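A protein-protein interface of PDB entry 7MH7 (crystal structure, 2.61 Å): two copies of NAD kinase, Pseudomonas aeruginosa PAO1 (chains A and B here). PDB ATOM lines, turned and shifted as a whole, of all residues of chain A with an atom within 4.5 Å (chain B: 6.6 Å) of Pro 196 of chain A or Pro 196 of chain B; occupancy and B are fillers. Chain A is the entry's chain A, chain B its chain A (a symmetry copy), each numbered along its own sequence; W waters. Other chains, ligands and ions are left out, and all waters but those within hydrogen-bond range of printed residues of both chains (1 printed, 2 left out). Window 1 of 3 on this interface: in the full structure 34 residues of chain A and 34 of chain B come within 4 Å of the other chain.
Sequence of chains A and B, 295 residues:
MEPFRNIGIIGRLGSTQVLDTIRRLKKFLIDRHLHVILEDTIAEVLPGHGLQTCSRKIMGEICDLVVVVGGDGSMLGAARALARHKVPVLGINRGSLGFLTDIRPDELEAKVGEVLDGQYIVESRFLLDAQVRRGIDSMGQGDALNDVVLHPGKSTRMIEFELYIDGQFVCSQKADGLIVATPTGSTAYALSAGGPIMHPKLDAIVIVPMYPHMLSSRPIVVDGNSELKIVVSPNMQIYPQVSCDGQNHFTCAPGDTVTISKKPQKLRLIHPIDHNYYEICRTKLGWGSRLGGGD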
ATOM      1  N   SER A 186     -14.176  22.680  -0.141  1.00  0.00           N
ATOM      2  CA  SER A 186     -13.162  22.896   0.885  1.00  0.00           C
ATOM      3  C   SER A 186     -13.212  21.837   1.978  1.00  0.00           C
ATOM      4  O   SER A 186     -12.207  21.622   2.664  1.00  0.00           O
ATOM      5  CB  SER A 186     -13.325  24.287   1.500  1.00  0.00           C
ATOM      6  OG  SER A 186     -14.533  24.381   2.237  1.00  0.00           O
ATOM      7  N   GLY A 194      -4.943  19.126   4.141  1.00  0.00           N
ATOM      8  CA  GLY A 194      -4.474  20.185   5.009  1.00  0.00           C
ATOM      9  C   GLY A 194      -5.150  21.526   4.821  1.00  0.00           C
ATOM     10  O   GLY A 194      -4.828  22.468   5.554  1.00  0.00           O
ATOM     11  N   GLY A 195      -6.075  21.642   3.870  1.00  0.00           N
ATOM     12  CA  GLY A 195      -6.728  22.898   3.594  1.00  0.00           C
ATOM     13  C   GLY A 195      -7.700  23.308   4.681  1.00  0.00           C
ATOM     14  O   GLY A 195      -8.088  22.509   5.539  1.00  0.00           O
ATOM     15  N   PRO A 196      -8.108  24.573   4.666  1.00  0.00           N
ATOM     16  CA  PRO A 196      -9.054  25.066   5.665  1.00  0.00           C
ATOM     17  C   PRO A 196     -10.499  24.893   5.218  1.00  0.00           C
ATOM     18  O   PRO A 196     -10.802  24.677   4.043  1.00  0.00           O
ATOM     19  CB  PRO A 196      -8.695  26.554   5.759  1.00  0.00           C
ATOM     20  CG  PRO A 196      -8.303  26.893   4.355  1.00  0.00           C
ATOM     21  CD  PRO A 196      -7.626  25.656   3.790  1.00  0.00           C
ATOM     22  N   ILE A 197     -11.396  24.991   6.193  1.00  0.00           N
ATOM     23  CA  ILE A 197     -12.823  25.040   5.909  1.00  0.00           C
ATOM     24  C   ILE A 197     -13.181  26.459   5.490  1.00  0.00           C
ATOM     25  O   ILE A 197     -12.803  27.430   6.156  1.00  0.00           O
ATOM     26  CB  ILE A 197     -13.639  24.599   7.133  1.00  0.00           C
ATOM     27  CG1 ILE A 197     -13.238  23.188   7.565  1.00  0.00           C
ATOM     28  CG2 ILE A 197     -15.128  24.656   6.830  1.00  0.00           C
ATOM     29  CD1 ILE A 197     -13.939  22.716   8.816  1.00  0.00           C
ATOM     30  N   MET A 198     -13.900  26.587   4.378  1.00  0.00           N
ATOM     31  CA  MET A 198     -14.338  27.884   3.878  1.00  0.00           C
ATOM     32  C   MET A 198     -15.856  27.945   3.941  1.00  0.00           C
ATOM     33  O   MET A 198     -16.539  27.076   3.387  1.00  0.00           O
ATOM     34  CB  MET A 198     -13.838  28.125   2.452  1.00  0.00           C
ATOM     35  CG  MET A 198     -12.322  28.237   2.340  1.00  0.00           C
ATOM     36  SD  MET A 198     -11.791  29.024   0.806  1.00  0.00           S
ATOM     37  CE  MET A 198     -12.646  28.021  -0.405  1.00  0.00           C
ATOM     38  N   VAL A 206      -9.596  28.188  -2.713  1.00  0.00           N
ATOM     39  CA  VAL A 206      -8.447  27.718  -1.947  1.00  0.00           C
ATOM     40  C   VAL A 206      -7.594  26.819  -2.833  1.00  0.00           C
ATOM     41  O   VAL A 206      -8.113  25.975  -3.573  1.00  0.00           O
ATOM     42  CB  VAL A 206      -8.881  26.995  -0.654  1.00  0.00           C
ATOM     43  CG1 VAL A 206      -9.699  25.747  -0.964  1.00  0.00           C
ATOM     44  CG2 VAL A 206      -7.670  26.658   0.196  1.00  0.00           C
ATOM     45  N   PRO A 219      -1.367  26.095   1.925  1.00  0.00           N
ATOM     46  CA  PRO A 219      -2.544  26.496   1.147  1.00  0.00           C
ATOM     47  C   PRO A 219      -2.685  28.008   1.056  1.00  0.00           C
ATOM     48  O   PRO A 219      -2.328  28.747   1.976  1.00  0.00           O
ATOM     49  CB  PRO A 219      -3.712  25.875   1.921  1.00  0.00           C
ATOM     50  CG  PRO A 219      -3.109  24.748   2.681  1.00  0.00           C
ATOM     51  CD  PRO A 219      -1.732  25.211   3.049  1.00  0.00           C
ATOM     52  N   VAL A 221      -5.566  31.088  -0.026  1.00  0.00           N
ATOM     53  CA  VAL A 221      -6.957  31.446  -0.275  1.00  0.00           C
ATOM     54  C   VAL A 221      -6.961  32.776  -1.011  1.00  0.00           C
ATOM     55  O   VAL A 221      -6.409  33.767  -0.516  1.00  0.00           O
ATOM     56  CB  VAL A 221      -7.775  31.530   1.023  1.00  0.00           C
ATOM     57  CG1 VAL A 221      -9.254  31.621   0.701  1.00  0.00           C
ATOM     58  CG2 VAL A 221      -7.491  30.331   1.910  1.00  0.00           C
ATOM     59  N   SER B 186      -2.425  36.421   8.453  1.00  0.00           N
ATOM     60  CA  SER B 186      -2.511  35.023   8.050  1.00  0.00           C
ATOM     61  C   SER B 186      -1.139  34.395   7.845  1.00  0.00           C
ATOM     62  O   SER B 186      -1.014  33.168   7.919  1.00  0.00           O
ATOM     63  CB  SER B 186      -3.338  34.894   6.770  1.00  0.00           C
ATOM     64  OG  SER B 186      -2.672  35.490   5.669  1.00  0.00           O
ATOM     65  N   THR B 187      -0.112  35.203   7.593  1.00  0.00           N
ATOM     66  CA  THR B 187       1.244  34.709   7.401  1.00  0.00           C
ATOM     67  C   THR B 187       2.054  34.676   8.690  1.00  0.00           C
ATOM     68  O   THR B 187       3.212  34.247   8.664  1.00  0.00           O
ATOM     69  CB  THR B 187       1.974  35.567   6.363  1.00  0.00           C
ATOM     70  OG1 THR B 187       1.860  36.952   6.720  1.00  0.00           O
ATOM     71  CG2 THR B 187       1.379  35.350   4.977  1.00  0.00           C
ATOM     72  N   ALA B 190      -0.809  32.505  12.714  1.00  0.00           N
ATOM     73  CA  ALA B 190      -1.771  31.575  12.131  1.00  0.00           C
ATOM     74  C   ALA B 190      -1.100  30.613  11.159  1.00  0.00           C
ATOM     75  O   ALA B 190      -1.494  29.445  11.061  1.00  0.00           O
ATOM     76  CB  ALA B 190      -2.889  32.349  11.435  1.00  0.00           C
ATOM     77  N   LEU B 191      -0.079  31.083  10.437  1.00  0.00           N
ATOM     78  CA  LEU B 191       0.632  30.202   9.516  1.00  0.00           C
ATOM     79  C   LEU B 191       1.430  29.145  10.271  1.00  0.00           C
ATOM     80  O   LEU B 191       1.514  27.993   9.833  1.00  0.00           O
ATOM     81  CB  LEU B 191       1.546  31.018   8.605  1.00  0.00           C
ATOM     82  CG  LEU B 191       2.174  30.240   7.450  1.00  0.00           C
ATOM     83  CD1 LEU B 191       1.094  29.745   6.499  1.00  0.00           C
ATOM     84  CD2 LEU B 191       3.196  31.093   6.715  1.00  0.00           C
ATOM     85  N   GLY B 194      -0.843  26.184  11.436  1.00  0.00           N
ATOM     86  CA  GLY B 194      -1.505  25.372  10.437  1.00  0.00           C
ATOM     87  C   GLY B 194      -2.462  26.113   9.529  1.00  0.00           C
ATOM     88  O   GLY B 194      -3.036  25.493   8.627  1.00  0.00           O
ATOM     89  N   GLY B 195      -2.650  27.416   9.732  1.00  0.00           N
ATOM     90  CA  GLY B 195      -3.583  28.183   8.944  1.00  0.00           C
ATOM     91  C   GLY B 195      -3.108  28.406   7.522  1.00  0.00           C
ATOM     92  O   GLY B 195      -1.936  28.204   7.192  1.00  0.00           O
ATOM     93  N   PRO B 196      -4.020  28.824   6.651  1.00  0.00           N
ATOM     94  CA  PRO B 196      -3.661  29.081   5.258  1.00  0.00           C
ATOM     95  C   PRO B 196      -3.207  30.517   5.038  1.00  0.00           C
ATOM     96  O   PRO B 196      -3.436  31.410   5.857  1.00  0.00           O
ATOM     97  CB  PRO B 196      -4.979  28.815   4.519  1.00  0.00           C
ATOM     98  CG  PRO B 196      -6.010  29.291   5.494  1.00  0.00           C
ATOM     99  CD  PRO B 196      -5.469  28.974   6.877  1.00  0.00           C
ATOM    100  N   ILE B 197      -2.549  30.723   3.904  1.00  0.00           N
ATOM    101  CA  ILE B 197      -2.214  32.066   3.454  1.00  0.00           C
ATOM    102  C   ILE B 197      -3.447  32.677   2.804  1.00  0.00           C
ATOM    103  O   ILE B 197      -4.093  32.048   1.957  1.00  0.00           O
ATOM    104  CB  ILE B 197      -1.028  32.036   2.478  1.00  0.00           C
ATOM    105  CG1 ILE B 197       0.189  31.383   3.133  1.00  0.00           C
ATOM    106  CG2 ILE B 197      -0.686  33.442   2.010  1.00  0.00           C
ATOM    107  CD1 ILE B 197       1.372  31.241   2.205  1.00  0.00           C
ATOM    108  N   MET B 198      -3.788  33.899   3.205  1.00  0.00           N
ATOM    109  CA  MET B 198      -4.928  34.614   2.645  1.00  0.00           C
ATOM    110  C   MET B 198      -4.419  35.840   1.903  1.00  0.00           C
ATOM    111  O   MET B 198      -3.701  36.665   2.480  1.00  0.00           O
ATOM    112  CB  MET B 198      -5.925  35.007   3.737  1.00  0.00           C
ATOM    113  CG  MET B 198      -6.596  33.820   4.415  1.00  0.00           C
ATOM    114  SD  MET B 198      -8.105  34.278   5.292  1.00  0.00           S
ATOM    115  CE  MET B 198      -7.503  35.604   6.334  1.00  0.00           C
ATOM    116  N   VAL B 206      -9.716  34.371   9.204  1.00  0.00           N
ATOM    117  CA  VAL B 206      -9.395  32.966   9.425  1.00  0.00           C
ATOM    118  C   VAL B 206      -9.335  32.701  10.925  1.00  0.00           C
ATOM    119  O   VAL B 206      -8.777  33.495  11.691  1.00  0.00           O
ATOM    120  CB  VAL B 206      -8.079  32.564   8.725  1.00  0.00           C
ATOM    121  CG1 VAL B 206      -6.894  33.344   9.281  1.00  0.00           C
ATOM    122  CG2 VAL B 206      -7.853  31.068   8.841  1.00  0.00           C
ATOM    123  N   VAL B 208      -8.110  29.899  13.626  1.00  0.00           N
ATOM    124  CA  VAL B 208      -7.170  28.788  13.702  1.00  0.00           C
ATOM    125  C   VAL B 208      -7.094  28.297  15.144  1.00  0.00           C
ATOM    126  O   VAL B 208      -6.732  29.064  16.040  1.00  0.00           O
ATOM    127  CB  VAL B 208      -5.775  29.184  13.191  1.00  0.00           C
ATOM    128  CG1 VAL B 208      -4.818  28.013  13.320  1.00  0.00           C
ATOM    129  CG2 VAL B 208      -5.856  29.656  11.747  1.00  0.00           C
ATOM    130  N   ARG B 218     -10.166  22.023  12.570  1.00  0.00           N
ATOM    131  CA  ARG B 218      -9.417  22.599  11.467  1.00  0.00           C
ATOM    132  C   ARG B 218      -9.725  24.084  11.321  1.00  0.00           C
ATOM    133  O   ARG B 218     -10.759  24.566  11.798  1.00  0.00           O
ATOM    134  CB  ARG B 218      -9.747  21.866  10.158  1.00  0.00           C
ATOM    135  CG  ARG B 218      -9.571  20.351  10.224  1.00  0.00           C
ATOM    136  CD  ARG B 218      -8.136  19.898   9.948  1.00  0.00           C
ATOM    137  NE  ARG B 218      -7.176  20.387  10.931  1.00  0.00           N
ATOM    138  CZ  ARG B 218      -6.188  21.229  10.659  1.00  0.00           C
ATOM    139  NH1 ARG B 218      -5.978  21.675   9.432  1.00  0.00           N
ATOM    140  NH2 ARG B 218      -5.385  21.626  11.642  1.00  0.00           N
ATOM    141  N   PRO B 219      -8.838  24.850  10.683  1.00  0.00           N
ATOM    142  CA  PRO B 219      -9.098  26.281  10.497  1.00  0.00           C
ATOM    143  C   PRO B 219     -10.342  26.535   9.657  1.00  0.00           C
ATOM    144  O   PRO B 219     -10.677  25.769   8.751  1.00  0.00           O
ATOM    145  CB  PRO B 219      -7.837  26.784   9.785  1.00  0.00           C
ATOM    146  CG  PRO B 219      -6.782  25.796  10.139  1.00  0.00           C
ATOM    147  CD  PRO B 219      -7.487  24.476  10.222  1.00  0.00           C
ATOM    148  N   ILE B 220     -11.032  27.627   9.979  1.00  0.00           N
ATOM    149  CA  ILE B 220     -12.204  28.074   9.238  1.00  0.00           C
ATOM    150  C   ILE B 220     -11.921  29.462   8.683  1.00  0.00           C
ATOM    151  O   ILE B 220     -11.316  30.299   9.361  1.00  0.00           O
ATOM    152  CB  ILE B 220     -13.472  28.098  10.117  1.00  0.00           C
ATOM    153  CG1 ILE B 220     -13.518  26.881  11.041  1.00  0.00           C
ATOM    154  CG2 ILE B 220     -14.724  28.153   9.248  1.00  0.00           C
ATOM    155  CD1 ILE B 220     -13.359  27.230  12.504  1.00  0.00           C
ATOM    156  N   VAL B 221     -12.358  29.700   7.450  1.00  0.00           N
ATOM    157  CA  VAL B 221     -12.276  31.012   6.819  1.00  0.00           C
ATOM    158  C   VAL B 221     -13.698  31.500   6.597  1.00  0.00           C
ATOM    159  O   VAL B 221     -14.497  30.824   5.936  1.00  0.00           O
ATOM    160  CB  VAL B 221     -11.493  30.972   5.498  1.00  0.00           C
ATOM    161  CG1 VAL B 221     -11.191  32.382   5.029  1.00  0.00           C
ATOM    162  CG2 VAL B 221     -10.211  30.175   5.662  1.00  0.00           C
HETATM  163  O   HOH W   1      -5.011  25.355   6.366  1.00  0.00           O
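Of chain B, only Pro 196, Pro 219 and Val 221 come within 4 Å of Pro 196 of chain A.
Pro 196 of chain B touches just these residues of chain A: Pro 196 (3.5 Å), Pro 219 (3.6 Å) and Val 221 (3.9 Å).
Of the printed residues of chain A, Ile 197 of chain B touches Pro 219 and Val 221.
Of the printed residues of chain A, Met 198 of chain B touches Val 221 (3.6 Å).
Arg 218 of chain B touches none of the printed residues of chain A.
The nearest printed residue of chain A that does not touch Pro 196 of chain B is Val 206 of chain A (5.5 Å).
The nearest printed residue of chain A that does not touch Val 221 of chain B is Val 221 of chain A (4.6 Å).
O of Pro 219 of chain B is in hydrogen-bond range of N of Ile 197 of chain A, 2.8 Å away.
The backbone carbonyl oxygen (O) of Ile 197 of chain A is in hydrogen-bond range of the backbone NH (N) of Val 221 of chain B (2.7 Å).
The backbone carbonyl oxygen (O) of Pro 219 of chain A lies within hydrogen-bond range of the backbone NH (N) of Ile 197 of chain B (2.8 Å).
O of Ile 197 of chain B sits at hydrogen-bond distance from N of Val 221 of chain A, at 2.7 Å.
Hydrophobic or aromatic side chains of chain A that line the printed part of chain B: Pro 196, Ile 197 and Val 221.
Printed residues of chain B that touch a printed residue of chain A: Pro 196, Ile 197, Met 198, Pro 219, Ile 220 and Val 221.
Among the printed residues, no Asp or Glu carboxylate lies within 4 Å of a Lys or Arg side-chain nitrogen of the other chain.
N of Met 198 of chain A lies within hydrogen-bond range of OG of Ser 186 of chain A.
The backbone NH of Met 198 of chain B lies within hydrogen-bond range of the side-chain hydroxyl of Ser 186 of chain B.
Pro 196 of chain A touches Pro 196 of chain B (CG to CG, 3.5 Å).
Pro 196 of chain A touches Pro 219 of chain B.
Val 221 of chain B touches Pro 196 of chain A (CG2 to CB, 3.9 Å).
Ile 220 of chain B touches Ile 197 of chain A.
Met 198 of chain A touches Val 221 of chain B (CA to O, 3.6 Å).
CA of Pro 196 of chain B touches O of Pro 219 of chain A, at 3.6 Å.
Val 221 of chain A touches Pro 196 of chain B.
CA of Met 198 of chain B touches O of Val 221 of chain A, 3.6 Å away.
Pro 196 of chain A touches its own counterpart, Pro 196 of chain B.
Pro 196 of chain A touches Pro 219 of chain B, and with the chains exchanged Pro 219 of chain A touches Pro 196 of chain B.
Ile 197 of chain A touches Val 221 of chain B, and with the chains exchanged Val 221 of chain A touches Ile 197 of chain B.
Met 198 of chain A touches Val 221 of chain B, and with the chains exchanged Val 221 of chain A touches Met 198 of chain B.
9 positions are printed for both chains.
Of the 12 pairs that touch across the chains among the printed residues, 11 have their exchanged pair printed and touching as well.
Water W1 lies within hydrogen-bond range of the backbone carbonyl oxygen of Gly 194 of chain A and the backbone carbonyl oxygen of Gly 194 of chain B.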
